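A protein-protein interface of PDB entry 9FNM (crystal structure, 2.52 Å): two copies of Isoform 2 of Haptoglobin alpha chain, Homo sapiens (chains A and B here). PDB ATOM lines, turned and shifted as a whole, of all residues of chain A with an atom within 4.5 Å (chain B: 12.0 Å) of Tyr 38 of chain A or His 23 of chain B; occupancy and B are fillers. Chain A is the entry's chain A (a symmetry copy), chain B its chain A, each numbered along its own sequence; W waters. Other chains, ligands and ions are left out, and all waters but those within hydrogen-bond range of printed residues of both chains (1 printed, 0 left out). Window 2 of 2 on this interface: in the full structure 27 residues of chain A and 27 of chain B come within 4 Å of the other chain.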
ATOM      1  N   CYS A  34      12.643 -27.161   4.537  1.00  0.00           N
ATOM      2  CA  CYS A  34      11.876 -28.315   4.098  1.00  0.00           C
ATOM      3  C   CYS A  34      12.787 -29.332   3.432  1.00  0.00           C
ATOM      4  O   CYS A  34      13.733 -28.970   2.728  1.00  0.00           O
ATOM      5  CB  CYS A  34      10.767 -27.904   3.131  1.00  0.00           C
ATOM      6  SG  CYS A  34       9.573 -26.773   3.857  1.00  0.00           S
ATOM      7  N   LYS A  35      12.500 -30.606   3.667  1.00  0.00           N
ATOM      8  CA  LYS A  35      13.192 -31.657   2.946  1.00  0.00           C
ATOM      9  C   LYS A  35      12.710 -31.701   1.501  1.00  0.00           C
ATOM     10  O   LYS A  35      11.771 -31.004   1.104  1.00  0.00           O
ATOM     11  CB  LYS A  35      12.953 -33.013   3.608  1.00  0.00           C
ATOM     12  CG  LYS A  35      12.830 -32.967   5.119  1.00  0.00           C
ATOM     13  CD  LYS A  35      12.565 -34.354   5.690  1.00  0.00           C
ATOM     14  CE  LYS A  35      12.454 -34.320   7.205  1.00  0.00           C
ATOM     15  NZ  LYS A  35      12.326 -35.688   7.780  1.00  0.00           N
ATOM     16  N   ASN A  36      13.369 -32.532   0.702  1.00  0.00           N
ATOM     17  CA  ASN A  36      12.789 -32.922  -0.573  1.00  0.00           C
ATOM     18  C   ASN A  36      11.539 -33.756  -0.311  1.00  0.00           C
ATOM     19  O   ASN A  36      11.479 -34.537   0.644  1.00  0.00           O
ATOM     20  CB  ASN A  36      13.797 -33.721  -1.397  1.00  0.00           C
ATOM     21  CG  ASN A  36      15.225 -33.508  -0.937  1.00  0.00           C
ATOM     22  OD1 ASN A  36      15.629 -32.391  -0.612  1.00  0.00           O
ATOM     23  ND2 ASN A  36      15.998 -34.586  -0.900  1.00  0.00           N
ATOM     24  N   TYR A  37      10.522 -33.584  -1.153  1.00  0.00           N
ATOM     25  CA  TYR A  37      10.557 -32.699  -2.309  1.00  0.00           C
ATOM     26  C   TYR A  37       9.612 -31.530  -2.061  1.00  0.00           C
ATOM     27  O   TYR A  37       8.601 -31.387  -2.746  1.00  0.00           O
ATOM     28  CB  TYR A  37      10.143 -33.449  -3.583  1.00  0.00           C
ATOM     29  CG  TYR A  37      11.047 -34.603  -3.982  1.00  0.00           C
ATOM     30  CD1 TYR A  37      11.347 -35.627  -3.087  1.00  0.00           C
ATOM     31  CD2 TYR A  37      11.577 -34.679  -5.261  1.00  0.00           C
ATOM     32  CE1 TYR A  37      12.166 -36.673  -3.444  1.00  0.00           C
ATOM     33  CE2 TYR A  37      12.394 -35.729  -5.630  1.00  0.00           C
ATOM     34  CZ  TYR A  37      12.686 -36.723  -4.717  1.00  0.00           C
ATOM     35  OH  TYR A  37      13.499 -37.773  -5.073  1.00  0.00           O
ATOM     36  N   TYR A  38       9.943 -30.696  -1.078  1.00  0.00           N
ATOM     37  CA  TYR A  38       9.020 -29.698  -0.556  1.00  0.00           C
ATOM     38  C   TYR A  38       9.650 -28.312  -0.588  1.00  0.00           C
ATOM     39  O   TYR A  38      10.857 -28.151  -0.788  1.00  0.00           O
ATOM     40  CB  TYR A  38       8.588 -30.049   0.876  1.00  0.00           C
ATOM     41  CG  TYR A  38       7.729 -31.285   0.962  1.00  0.00           C
ATOM     42  CD1 TYR A  38       8.291 -32.553   0.896  1.00  0.00           C
ATOM     43  CD2 TYR A  38       6.351 -31.186   1.107  1.00  0.00           C
ATOM     44  CE1 TYR A  38       7.503 -33.689   0.968  1.00  0.00           C
ATOM     45  CE2 TYR A  38       5.558 -32.315   1.183  1.00  0.00           C
ATOM     46  CZ  TYR A  38       6.137 -33.561   1.113  1.00  0.00           C
ATOM     47  OH  TYR A  38       5.345 -34.683   1.190  1.00  0.00           O
ATOM     48  N   LYS A  39       8.804 -27.302  -0.384  1.00  0.00           N
ATOM     49  CA  LYS A  39       9.227 -25.912  -0.347  1.00  0.00           C
ATOM     50  C   LYS A  39       8.634 -25.232   0.880  1.00  0.00           C
ATOM     51  O   LYS A  39       7.573 -25.619   1.374  1.00  0.00           O
ATOM     52  CB  LYS A  39       8.813 -25.156  -1.618  1.00  0.00           C
ATOM     53  CG  LYS A  39       7.309 -25.015  -1.794  1.00  0.00           C
ATOM     54  CD  LYS A  39       6.970 -24.028  -2.901  1.00  0.00           C
ATOM     55  CE  LYS A  39       7.492 -24.501  -4.245  1.00  0.00           C
ATOM     56  NZ  LYS A  39       7.089 -23.580  -5.343  1.00  0.00           N
ATOM     57  N   CYS A  68       5.518 -26.737   4.991  1.00  0.00           N
ATOM     58  CA  CYS A  68       6.272 -27.363   3.911  1.00  0.00           C
ATOM     59  C   CYS A  68       5.281 -27.874   2.874  1.00  0.00           C
ATOM     60  O   CYS A  68       4.551 -28.839   3.124  1.00  0.00           O
ATOM     61  CB  CYS A  68       7.165 -28.486   4.433  1.00  0.00           C
ATOM     62  SG  CYS A  68       8.633 -27.875   5.278  1.00  0.00           S
ATOM     63  N   GLU A  69       5.256 -27.220   1.720  1.00  0.00           N
ATOM     64  CA  GLU A  69       4.356 -27.571   0.634  1.00  0.00           C
ATOM     65  C   GLU A  69       5.112 -28.365  -0.422  1.00  0.00           C
ATOM     66  O   GLU A  69       6.292 -28.107  -0.678  1.00  0.00           O
ATOM     67  CB  GLU A  69       3.745 -26.313   0.014  1.00  0.00           C
ATOM     68  CG  GLU A  69       2.649 -26.571  -1.004  1.00  0.00           C
ATOM     69  CD  GLU A  69       2.245 -25.310  -1.741  1.00  0.00           C
ATOM     70  OE1 GLU A  69       2.858 -24.251  -1.485  1.00  0.00           O
ATOM     71  OE2 GLU A  69       1.319 -25.376  -2.575  1.00  0.00           O
ATOM     72  N   ALA A  70       4.429 -29.331  -1.028  1.00  0.00           N
ATOM     73  CA  ALA A  70       5.060 -30.173  -2.032  1.00  0.00           C
ATOM     74  C   ALA A  70       5.323 -29.388  -3.310  1.00  0.00           C
ATOM     75  O   ALA A  70       4.554 -28.506  -3.699  1.00  0.00           O
ATOM     76  CB  ALA A  70       4.185 -31.387  -2.338  1.00  0.00           C
ATOM     77  N   VAL A  71       6.430 -29.719  -3.963  1.00  0.00           N
ATOM     78  CA  VAL A  71       6.779 -29.098  -5.234  1.00  0.00           C
ATOM     79  C   VAL A  71       6.095 -29.863  -6.358  1.00  0.00           C
ATOM     80  O   VAL A  71       6.125 -31.099  -6.391  1.00  0.00           O
ATOM     81  CB  VAL A  71       8.303 -29.073  -5.426  1.00  0.00           C
ATOM     82  CG1 VAL A  71       8.665 -28.350  -6.705  1.00  0.00           C
ATOM     83  CG2 VAL A  71       8.967 -28.408  -4.235  1.00  0.00           C
ATOM     84  N   PRO B  19       8.839 -26.323  17.926  1.00  0.00           N
ATOM     85  CA  PRO B  19       7.854 -27.255  17.368  1.00  0.00           C
ATOM     86  C   PRO B  19       8.309 -27.781  16.015  1.00  0.00           C
ATOM     87  O   PRO B  19       8.918 -27.063  15.218  1.00  0.00           O
ATOM     88  CB  PRO B  19       6.583 -26.408  17.247  1.00  0.00           C
ATOM     89  CG  PRO B  19       6.801 -25.240  18.154  1.00  0.00           C
ATOM     90  CD  PRO B  19       8.275 -24.978  18.129  1.00  0.00           C
ATOM     91  N   GLU B  20       8.023 -29.053  15.770  1.00  0.00           N
ATOM     92  CA  GLU B  20       8.368 -29.683  14.508  1.00  0.00           C
ATOM     93  C   GLU B  20       7.235 -29.521  13.506  1.00  0.00           C
ATOM     94  O   GLU B  20       6.054 -29.524  13.865  1.00  0.00           O
ATOM     95  CB  GLU B  20       8.688 -31.164  14.714  1.00  0.00           C
ATOM     96  CG  GLU B  20       7.968 -31.793  15.897  1.00  0.00           C
ATOM     97  CD  GLU B  20       8.512 -33.165  16.244  1.00  0.00           C
ATOM     98  OE1 GLU B  20       8.456 -34.065  15.380  1.00  0.00           O
ATOM     99  OE2 GLU B  20       9.008 -33.339  17.378  1.00  0.00           O
ATOM    100  N   ILE B  21       7.609 -29.359  12.241  1.00  0.00           N
ATOM    101  CA  ILE B  21       6.652 -29.248  11.151  1.00  0.00           C
ATOM    102  C   ILE B  21       6.820 -30.451  10.236  1.00  0.00           C
ATOM    103  O   ILE B  21       7.912 -31.015  10.112  1.00  0.00           O
ATOM    104  CB  ILE B  21       6.819 -27.929  10.363  1.00  0.00           C
ATOM    105  CG1 ILE B  21       8.201 -27.857   9.708  1.00  0.00           C
ATOM    106  CG2 ILE B  21       6.609 -26.735  11.281  1.00  0.00           C
ATOM    107  CD1 ILE B  21       8.413 -26.608   8.871  1.00  0.00           C
ATOM    108  N   ALA B  22       5.720 -30.853   9.602  1.00  0.00           N
ATOM    109  CA  ALA B  22       5.753 -32.008   8.718  1.00  0.00           C
ATOM    110  C   ALA B  22       6.668 -31.744   7.530  1.00  0.00           C
ATOM    111  O   ALA B  22       6.641 -30.666   6.932  1.00  0.00           O
ATOM    112  CB  ALA B  22       4.343 -32.346   8.235  1.00  0.00           C
ATOM    113  N   HIS B  23       7.499 -32.736   7.207  1.00  0.00           N
ATOM    114  CA  HIS B  23       8.438 -32.683   6.088  1.00  0.00           C
ATOM    115  C   HIS B  23       9.423 -31.525   6.202  1.00  0.00           C
ATOM    116  O   HIS B  23      10.019 -31.112   5.203  1.00  0.00           O
ATOM    117  CB  HIS B  23       7.702 -32.620   4.745  1.00  0.00           C
ATOM    118  CG  HIS B  23       6.873 -33.832   4.457  1.00  0.00           C
ATOM    119  ND1 HIS B  23       5.499 -33.833   4.555  1.00  0.00           N
ATOM    120  CD2 HIS B  23       7.225 -35.084   4.083  1.00  0.00           C
ATOM    121  CE1 HIS B  23       5.038 -35.034   4.250  1.00  0.00           C
ATOM    122  NE2 HIS B  23       6.065 -35.812   3.960  1.00  0.00           N
ATOM    123  N   GLY B  24       9.608 -30.990   7.412  1.00  0.00           N
ATOM    124  CA  GLY B  24      10.574 -29.947   7.659  1.00  0.00           C
ATOM    125  C   GLY B  24      11.584 -30.383   8.709  1.00  0.00           C
ATOM    126  O   GLY B  24      11.437 -31.425   9.360  1.00  0.00           O
ATOM    127  N   TYR B  25      12.627 -29.571   8.857  1.00  0.00           N
ATOM    128  CA  TYR B  25      13.635 -29.812   9.877  1.00  0.00           C
ATOM    129  C   TYR B  25      14.228 -28.479  10.306  1.00  0.00           C
ATOM    130  O   TYR B  25      14.107 -27.467   9.610  1.00  0.00           O
ATOM    131  CB  TYR B  25      14.731 -30.765   9.378  1.00  0.00           C
ATOM    132  CG  TYR B  25      15.590 -30.207   8.264  1.00  0.00           C
ATOM    133  CD1 TYR B  25      15.185 -30.286   6.938  1.00  0.00           C
ATOM    134  CD2 TYR B  25      16.813 -29.611   8.537  1.00  0.00           C
ATOM    135  CE1 TYR B  25      15.971 -29.781   5.917  1.00  0.00           C
ATOM    136  CE2 TYR B  25      17.606 -29.102   7.523  1.00  0.00           C
ATOM    137  CZ  TYR B  25      17.181 -29.190   6.215  1.00  0.00           C
ATOM    138  OH  TYR B  25      17.966 -28.686   5.203  1.00  0.00           O
ATOM    139  N   VAL B  26      14.873 -28.492  11.468  1.00  0.00           N
ATOM    140  CA  VAL B  26      15.438 -27.294  12.071  1.00  0.00           C
ATOM    141  C   VAL B  26      16.950 -27.438  12.149  1.00  0.00           C
ATOM    142  O   VAL B  26      17.468 -28.523  12.435  1.00  0.00           O
ATOM    143  CB  VAL B  26      14.846 -27.030  13.473  1.00  0.00           C
ATOM    144  CG1 VAL B  26      13.390 -26.633  13.367  1.00  0.00           C
ATOM    145  CG2 VAL B  26      14.995 -28.261  14.357  1.00  0.00           C
ATOM    146  N   GLU B  27      17.655 -26.346  11.875  1.00  0.00           N
ATOM    147  CA  GLU B  27      19.063 -26.219  12.221  1.00  0.00           C
ATOM    148  C   GLU B  27      19.165 -25.240  13.382  1.00  0.00           C
ATOM    149  O   GLU B  27      18.565 -24.159  13.346  1.00  0.00           O
ATOM    150  CB  GLU B  27      19.913 -25.763  11.028  1.00  0.00           C
ATOM    151  CG  GLU B  27      19.722 -24.322  10.583  1.00  0.00           C
ATOM    152  CD  GLU B  27      20.919 -23.791   9.814  1.00  0.00           C
ATOM    153  OE1 GLU B  27      21.689 -24.608   9.264  1.00  0.00           O
ATOM    154  OE2 GLU B  27      21.094 -22.555   9.768  1.00  0.00           O
HETATM  155  O   HOH W   1       4.524 -28.386   7.124  1.00  0.00           O
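Among the printed residues, pairs that only touch across the chains: Cys 34 of chain A with His 23 of chain B (3.5 Å), Cys 34 of chain A with Tyr 25 of chain B (3.98 Å), Lys 35 of chain A with Gly 24 of chain B (3.7 Å), Cys 68 of chain A with Ile 21 of chain B (3.8 Å), Cys 68 of chain A with Ala 22 of chain B (3.4 Å) and Cys 68 of chain A with Gly 24 of chain B (3.7 Å).
Water W1 bridges the backbone NH of Cys 68 of chain A (2.9 Å) and the backbone carbonyl oxygen of Ala 22 of chain B (3.1 Å).
No position is printed for both chains.
Of the 9 pairs that touch across the chains among the printed residues, none has its exchanged pair printed and touching as well.
Hydrophobic or aromatic side chains of chain B within 4 Å of the printed part of chain A: Ile 21, His 23 and Tyr 25.
Hydrophobic or aromatic side chains of chain A that line the printed part of chain B: Tyr 38.
Among the printed residues, 9 pairs touch across the chains.
The backbone carbonyl oxygen of His 23 of chain B sits at hydrogen-bond distance from the backbone NH of Lys 35 of chain A (3.0 Å).
The side-chain hydroxyl (OH) of Tyr 38 of chain A lies within hydrogen-bond range of a ring nitrogen (NE2) of His 23 of chain B.
The side-chain sulfur (SG) of Cys 68 of chain A lies close to the backbone carbonyl oxygen (O) of His 23 of chain B, 3.5 Å away.
Cys 34 of chain A touches just these residues of chain B: His 23 and Tyr 25.
Of the printed residues of chain B, Lys 35 of chain A touches His 23 and Gly 24.
No residue of chain B comes within 4 Å of Asn 36 of chain A.
No residue of chain B comes within 4 Å of Lys 39 of chain A.
Printed residues of chain B within 4 Å of Cys 68 of chain A: Ile 21, Ala 22, His 23 and Gly 24.
Of chain A, only Cys 34 (3.5 Å), Lys 35 (3.0 Å), Tyr 38 (3.1 Å) and Cys 68 (3.5 Å) come within 4 Å of His 23 of chain B.
Of the printed residues of chain A, Gly 24 of chain B touches Lys 35 (3.7 Å) and Cys 68 (3.7 Å).
Val 26 of chain B touches none of the printed residues of chain A.
The nearest printed residue of chain A that does not touch His 23 of chain B is Asn 36 of chain A (5.5 Å).
The nearest printed residue of chain B that does not touch Lys 35 of chain A is Tyr 25 of chain B (4.01 Å).
The side-chain sulfur (SG) of Cys 34 of chain A is disulfide-bonded to the side-chain sulfur (SG) of Cys 68 of chain A, at 2.0 Å.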
